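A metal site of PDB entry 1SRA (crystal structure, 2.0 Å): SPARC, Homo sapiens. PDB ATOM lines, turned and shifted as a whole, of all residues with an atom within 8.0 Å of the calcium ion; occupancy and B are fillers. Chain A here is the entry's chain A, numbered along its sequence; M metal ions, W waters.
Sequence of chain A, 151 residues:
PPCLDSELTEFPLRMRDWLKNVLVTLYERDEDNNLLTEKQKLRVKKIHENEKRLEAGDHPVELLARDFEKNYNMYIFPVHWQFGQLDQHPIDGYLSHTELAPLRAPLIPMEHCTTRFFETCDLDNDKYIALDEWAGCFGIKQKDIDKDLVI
The side-chain carboxylate (OE1) of Glu 133 sits close to the backbone NH (N) of Ala 130, at 3.0 Å.
The side-chain carboxylate of Glu 133 lies close to the backbone NH of Leu 123.
The side-chain carboxylate of Asp 122 lies within hydrogen-bond range of the backbone NH of Lys 127, at 2.8 Å.
The side-chain carboxylate of Asp 122 sits close to the backbone NH of Asn 125, at 3.3 Å.
The nearest printed residue that does not touch the calcium ion is Ile 129 (4.5 Å).
The calcium ion is bound by OD1 of Asp 122 (2.3 Å), OD1 of Asp 126 (2.3 Å), OE1 of Glu 133 (2.4 Å), OD1 of Asp 124 (2.4 Å), water W1 (2.4 Å), O of Tyr 128 (2.4 Å) and OE2 of Glu 133 (2.7 Å).
Water W1 lies within hydrogen-bond range of OD2 of Asp 126 (2.5 Å) and OD2 of Asp 124 (3.4 Å).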
ATOM      1  N   TYR A  94       7.553 -11.250 -23.997  1.00  0.00           N
ATOM      2  CA  TYR A  94       8.629 -10.420 -23.440  1.00  0.00           C
ATOM      3  C   TYR A  94       8.670  -9.100 -24.216  1.00  0.00           C
ATOM      4  O   TYR A  94       8.198  -9.009 -25.353  1.00  0.00           O
ATOM      5  CB  TYR A  94      10.019 -11.061 -23.592  1.00  0.00           C
ATOM      6  CG  TYR A  94      10.150 -12.394 -22.922  1.00  0.00           C
ATOM      7  CD1 TYR A  94       9.686 -13.546 -23.570  1.00  0.00           C
ATOM      8  CD2 TYR A  94      10.597 -12.503 -21.593  1.00  0.00           C
ATOM      9  CE1 TYR A  94       9.656 -14.777 -22.907  1.00  0.00           C
ATOM     10  CE2 TYR A  94      10.569 -13.735 -20.920  1.00  0.00           C
ATOM     11  CZ  TYR A  94      10.095 -14.866 -21.586  1.00  0.00           C
ATOM     12  OH  TYR A  94      10.025 -16.095 -20.954  1.00  0.00           O
ATOM     13  N   LEU A  95       9.214  -8.072 -23.571  1.00  0.00           N
ATOM     14  CA  LEU A  95       9.345  -6.764 -24.204  1.00  0.00           C
ATOM     15  C   LEU A  95      10.810  -6.405 -24.248  1.00  0.00           C
ATOM     16  O   LEU A  95      11.481  -6.355 -23.225  1.00  0.00           O
ATOM     17  CB  LEU A  95       8.557  -5.692 -23.428  1.00  0.00           C
ATOM     18  CG  LEU A  95       7.045  -5.814 -23.280  1.00  0.00           C
ATOM     19  CD1 LEU A  95       6.529  -4.533 -22.674  1.00  0.00           C
ATOM     20  CD2 LEU A  95       6.392  -6.000 -24.633  1.00  0.00           C
ATOM     21  N   PHE A 118      12.307   0.642 -16.118  1.00  0.00           N
ATOM     22  CA  PHE A 118      12.272  -0.733 -16.593  1.00  0.00           C
ATOM     23  C   PHE A 118      13.435  -1.583 -16.194  1.00  0.00           C
ATOM     24  O   PHE A 118      13.260  -2.765 -15.957  1.00  0.00           O
ATOM     25  CB  PHE A 118      11.886  -0.831 -18.069  1.00  0.00           C
ATOM     26  CG  PHE A 118      10.423  -0.586 -18.288  1.00  0.00           C
ATOM     27  CD1 PHE A 118       9.487  -1.405 -17.673  1.00  0.00           C
ATOM     28  CD2 PHE A 118       9.987   0.549 -18.965  1.00  0.00           C
ATOM     29  CE1 PHE A 118       8.124  -1.101 -17.707  1.00  0.00           C
ATOM     30  CE2 PHE A 118       8.631   0.866 -19.000  1.00  0.00           C
ATOM     31  CZ  PHE A 118       7.701   0.036 -18.367  1.00  0.00           C
ATOM     32  N   GLU A 119      14.612  -0.962 -16.032  1.00  0.00           N
ATOM     33  CA  GLU A 119      15.804  -1.686 -15.572  1.00  0.00           C
ATOM     34  C   GLU A 119      15.412  -2.282 -14.205  1.00  0.00           C
ATOM     35  O   GLU A 119      15.726  -3.421 -13.879  1.00  0.00           O
ATOM     36  CB  GLU A 119      16.991  -0.721 -15.377  1.00  0.00           C
ATOM     37  N   CYS A 121      12.354  -3.180 -13.198  1.00  0.00           N
ATOM     38  CA  CYS A 121      11.410  -4.298 -13.285  1.00  0.00           C
ATOM     39  C   CYS A 121      12.067  -5.569 -13.822  1.00  0.00           C
ATOM     40  O   CYS A 121      11.494  -6.646 -13.730  1.00  0.00           O
ATOM     41  CB  CYS A 121      10.238  -3.925 -14.208  1.00  0.00           C
ATOM     42  SG  CYS A 121       9.624  -2.239 -14.003  1.00  0.00           S
ATOM     43  N   ASP A 122      13.239  -5.425 -14.442  1.00  0.00           N
ATOM     44  CA  ASP A 122      13.956  -6.562 -15.008  1.00  0.00           C
ATOM     45  C   ASP A 122      14.647  -7.329 -13.903  1.00  0.00           C
ATOM     46  O   ASP A 122      15.864  -7.248 -13.764  1.00  0.00           O
ATOM     47  CB  ASP A 122      15.002  -6.076 -16.005  1.00  0.00           C
ATOM     48  CG  ASP A 122      15.638  -7.211 -16.778  1.00  0.00           C
ATOM     49  OD1 ASP A 122      15.105  -8.346 -16.729  1.00  0.00           O
ATOM     50  OD2 ASP A 122      16.654  -6.970 -17.438  1.00  0.00           O
ATOM     51  N   LEU A 123      13.880  -8.143 -13.195  1.00  0.00           N
ATOM     52  CA  LEU A 123      14.391  -8.932 -12.068  1.00  0.00           C
ATOM     53  C   LEU A 123      15.447  -9.981 -12.393  1.00  0.00           C
ATOM     54  O   LEU A 123      16.303 -10.288 -11.545  1.00  0.00           O
ATOM     55  CB  LEU A 123      13.231  -9.556 -11.327  1.00  0.00           C
ATOM     56  CG  LEU A 123      12.210  -8.468 -10.988  1.00  0.00           C
ATOM     57  CD1 LEU A 123      11.023  -9.055 -10.270  1.00  0.00           C
ATOM     58  CD2 LEU A 123      12.845  -7.362 -10.166  1.00  0.00           C
ATOM     59  N   ASP A 124      15.415 -10.543 -13.595  1.00  0.00           N
ATOM     60  CA  ASP A 124      16.417 -11.550 -13.958  1.00  0.00           C
ATOM     61  C   ASP A 124      17.542 -11.016 -14.827  1.00  0.00           C
ATOM     62  O   ASP A 124      18.388 -11.753 -15.283  1.00  0.00           O
ATOM     63  CB  ASP A 124      15.760 -12.803 -14.554  1.00  0.00           C
ATOM     64  CG  ASP A 124      15.009 -12.525 -15.821  1.00  0.00           C
ATOM     65  OD1 ASP A 124      15.110 -11.393 -16.351  1.00  0.00           O
ATOM     66  OD2 ASP A 124      14.330 -13.441 -16.304  1.00  0.00           O
ATOM     67  N   ASN A 125      17.558  -9.709 -15.082  1.00  0.00           N
ATOM     68  CA  ASN A 125      18.644  -9.145 -15.848  1.00  0.00           C
ATOM     69  C   ASN A 125      18.874  -9.569 -17.263  1.00  0.00           C
ATOM     70  O   ASN A 125      19.945  -9.306 -17.791  1.00  0.00           O
ATOM     71  CB  ASN A 125      19.965  -9.323 -15.087  1.00  0.00           C
ATOM     72  CG  ASN A 125      20.260  -8.167 -14.149  1.00  0.00           C
ATOM     73  OD1 ASN A 125      19.679  -8.074 -13.065  1.00  0.00           O
ATOM     74  ND2 ASN A 125      21.197  -7.298 -14.556  1.00  0.00           N
ATOM     75  N   ASP A 126      17.875 -10.136 -17.930  1.00  0.00           N
ATOM     76  CA  ASP A 126      18.080 -10.538 -19.327  1.00  0.00           C
ATOM     77  C   ASP A 126      17.827  -9.382 -20.296  1.00  0.00           C
ATOM     78  O   ASP A 126      17.866  -9.590 -21.510  1.00  0.00           O
ATOM     79  CB  ASP A 126      17.217 -11.748 -19.696  1.00  0.00           C
ATOM     80  CG  ASP A 126      15.737 -11.481 -19.590  1.00  0.00           C
ATOM     81  OD1 ASP A 126      15.306 -10.415 -19.086  1.00  0.00           O
ATOM     82  OD2 ASP A 126      14.987 -12.385 -19.993  1.00  0.00           O
ATOM     83  N   LYS A 127      17.542  -8.184 -19.771  1.00  0.00           N
ATOM     84  CA  LYS A 127      17.270  -7.007 -20.610  1.00  0.00           C
ATOM     85  C   LYS A 127      15.919  -7.037 -21.353  1.00  0.00           C
ATOM     86  O   LYS A 127      15.685  -6.266 -22.281  1.00  0.00           O
ATOM     87  CB  LYS A 127      18.416  -6.785 -21.612  1.00  0.00           C
ATOM     88  CG  LYS A 127      19.614  -5.968 -21.096  1.00  0.00           C
ATOM     89  CD  LYS A 127      20.365  -6.601 -19.927  1.00  0.00           C
ATOM     90  CE  LYS A 127      21.518  -7.504 -20.383  1.00  0.00           C
ATOM     91  NZ  LYS A 127      22.330  -7.984 -19.212  1.00  0.00           N
ATOM     92  N   TYR A 128      15.060  -7.984 -20.989  1.00  0.00           N
ATOM     93  CA  TYR A 128      13.743  -8.092 -21.599  1.00  0.00           C
ATOM     94  C   TYR A 128      12.767  -8.031 -20.461  1.00  0.00           C
ATOM     95  O   TYR A 128      13.107  -8.407 -19.345  1.00  0.00           O
ATOM     96  CB  TYR A 128      13.581  -9.432 -22.340  1.00  0.00           C
ATOM     97  CG  TYR A 128      14.154  -9.428 -23.748  1.00  0.00           C
ATOM     98  CD1 TYR A 128      15.510  -9.290 -23.950  1.00  0.00           C
ATOM     99  CD2 TYR A 128      13.326  -9.594 -24.862  1.00  0.00           C
ATOM    100  CE1 TYR A 128      16.039  -9.324 -25.224  1.00  0.00           C
ATOM    101  CE2 TYR A 128      13.836  -9.625 -26.121  1.00  0.00           C
ATOM    102  CZ  TYR A 128      15.191  -9.500 -26.303  1.00  0.00           C
ATOM    103  OH  TYR A 128      15.710  -9.600 -27.568  1.00  0.00           O
ATOM    104  N   ILE A 129      11.552  -7.568 -20.710  1.00  0.00           N
ATOM    105  CA  ILE A 129      10.583  -7.499 -19.625  1.00  0.00           C
ATOM    106  C   ILE A 129       9.510  -8.562 -19.874  1.00  0.00           C
ATOM    107  O   ILE A 129       8.755  -8.455 -20.828  1.00  0.00           O
ATOM    108  CB  ILE A 129       9.935  -6.052 -19.515  1.00  0.00           C
ATOM    109  CG1 ILE A 129      11.009  -4.958 -19.358  1.00  0.00           C
ATOM    110  CG2 ILE A 129       8.949  -5.976 -18.353  1.00  0.00           C
ATOM    111  CD1 ILE A 129      11.866  -5.047 -18.129  1.00  0.00           C
ATOM    112  N   ALA A 130       9.426  -9.551 -18.990  1.00  0.00           N
ATOM    113  CA  ALA A 130       8.404 -10.600 -19.138  1.00  0.00           C
ATOM    114  C   ALA A 130       7.081 -10.044 -18.624  1.00  0.00           C
ATOM    115  O   ALA A 130       7.088  -9.072 -17.872  1.00  0.00           O
ATOM    116  CB  ALA A 130       8.813 -11.835 -18.293  1.00  0.00           C
ATOM    117  N   LEU A 131       5.965 -10.644 -19.007  1.00  0.00           N
ATOM    118  CA  LEU A 131       4.670 -10.179 -18.535  1.00  0.00           C
ATOM    119  C   LEU A 131       4.574 -10.116 -17.015  1.00  0.00           C
ATOM    120  O   LEU A 131       3.972  -9.187 -16.455  1.00  0.00           O
ATOM    121  CB  LEU A 131       3.531 -11.075 -19.038  1.00  0.00           C
ATOM    122  CG  LEU A 131       2.137 -10.765 -18.457  1.00  0.00           C
ATOM    123  CD1 LEU A 131       1.644  -9.388 -18.924  1.00  0.00           C
ATOM    124  CD2 LEU A 131       1.144 -11.842 -18.839  1.00  0.00           C
ATOM    125  N   ASP A 132       5.129 -11.104 -16.329  1.00  0.00           N
ATOM    126  CA  ASP A 132       5.027 -11.076 -14.881  1.00  0.00           C
ATOM    127  C   ASP A 132       5.917  -9.989 -14.277  1.00  0.00           C
ATOM    128  O   ASP A 132       5.585  -9.446 -13.244  1.00  0.00           O
ATOM    129  CB  ASP A 132       5.317 -12.452 -14.271  1.00  0.00           C
ATOM    130  CG  ASP A 132       6.771 -12.860 -14.398  1.00  0.00           C
ATOM    131  OD1 ASP A 132       7.589 -12.414 -13.558  1.00  0.00           O
ATOM    132  OD2 ASP A 132       7.108 -13.645 -15.309  1.00  0.00           O
ATOM    133  N   GLU A 133       7.047  -9.678 -14.910  1.00  0.00           N
ATOM    134  CA  GLU A 133       7.912  -8.618 -14.405  1.00  0.00           C
ATOM    135  C   GLU A 133       7.208  -7.270 -14.667  1.00  0.00           C
ATOM    136  O   GLU A 133       7.404  -6.306 -13.941  1.00  0.00           O
ATOM    137  CB  GLU A 133       9.273  -8.622 -15.099  1.00  0.00           C
ATOM    138  CG  GLU A 133      10.199  -9.810 -14.781  1.00  0.00           C
ATOM    139  CD  GLU A 133      11.505  -9.795 -15.594  1.00  0.00           C
ATOM    140  OE1 GLU A 133      11.475  -9.458 -16.808  1.00  0.00           O
ATOM    141  OE2 GLU A 133      12.560 -10.129 -15.032  1.00  0.00           O
ATOM    142  N   TRP A 134       6.415  -7.202 -15.738  1.00  0.00           N
ATOM    143  CA  TRP A 134       5.687  -5.996 -16.103  1.00  0.00           C
ATOM    144  C   TRP A 134       4.535  -5.734 -15.140  1.00  0.00           C
ATOM    145  O   TRP A 134       4.419  -4.640 -14.579  1.00  0.00           O
ATOM    146  CB  TRP A 134       5.142  -6.092 -17.520  1.00  0.00           C
ATOM    147  CG  TRP A 134       4.107  -5.029 -17.920  1.00  0.00           C
ATOM    148  CD1 TRP A 134       2.748  -5.084 -17.714  1.00  0.00           C
ATOM    149  CD2 TRP A 134       4.337  -3.862 -18.728  1.00  0.00           C
ATOM    150  NE1 TRP A 134       2.127  -4.057 -18.361  1.00  0.00           N
ATOM    151  CE2 TRP A 134       3.076  -3.285 -18.981  1.00  0.00           C
ATOM    152  CE3 TRP A 134       5.476  -3.257 -19.258  1.00  0.00           C
ATOM    153  CZ2 TRP A 134       2.932  -2.131 -19.760  1.00  0.00           C
ATOM    154  CZ3 TRP A 134       5.318  -2.128 -20.034  1.00  0.00           C
ATOM    155  CH2 TRP A 134       4.058  -1.574 -20.268  1.00  0.00           C
HETATM  156 CA    CA M   1      13.669  -9.938 -17.531  1.00  0.00          CA
HETATM  157  O   HOH W   1      12.791 -11.741 -18.881  1.00  0.00           O
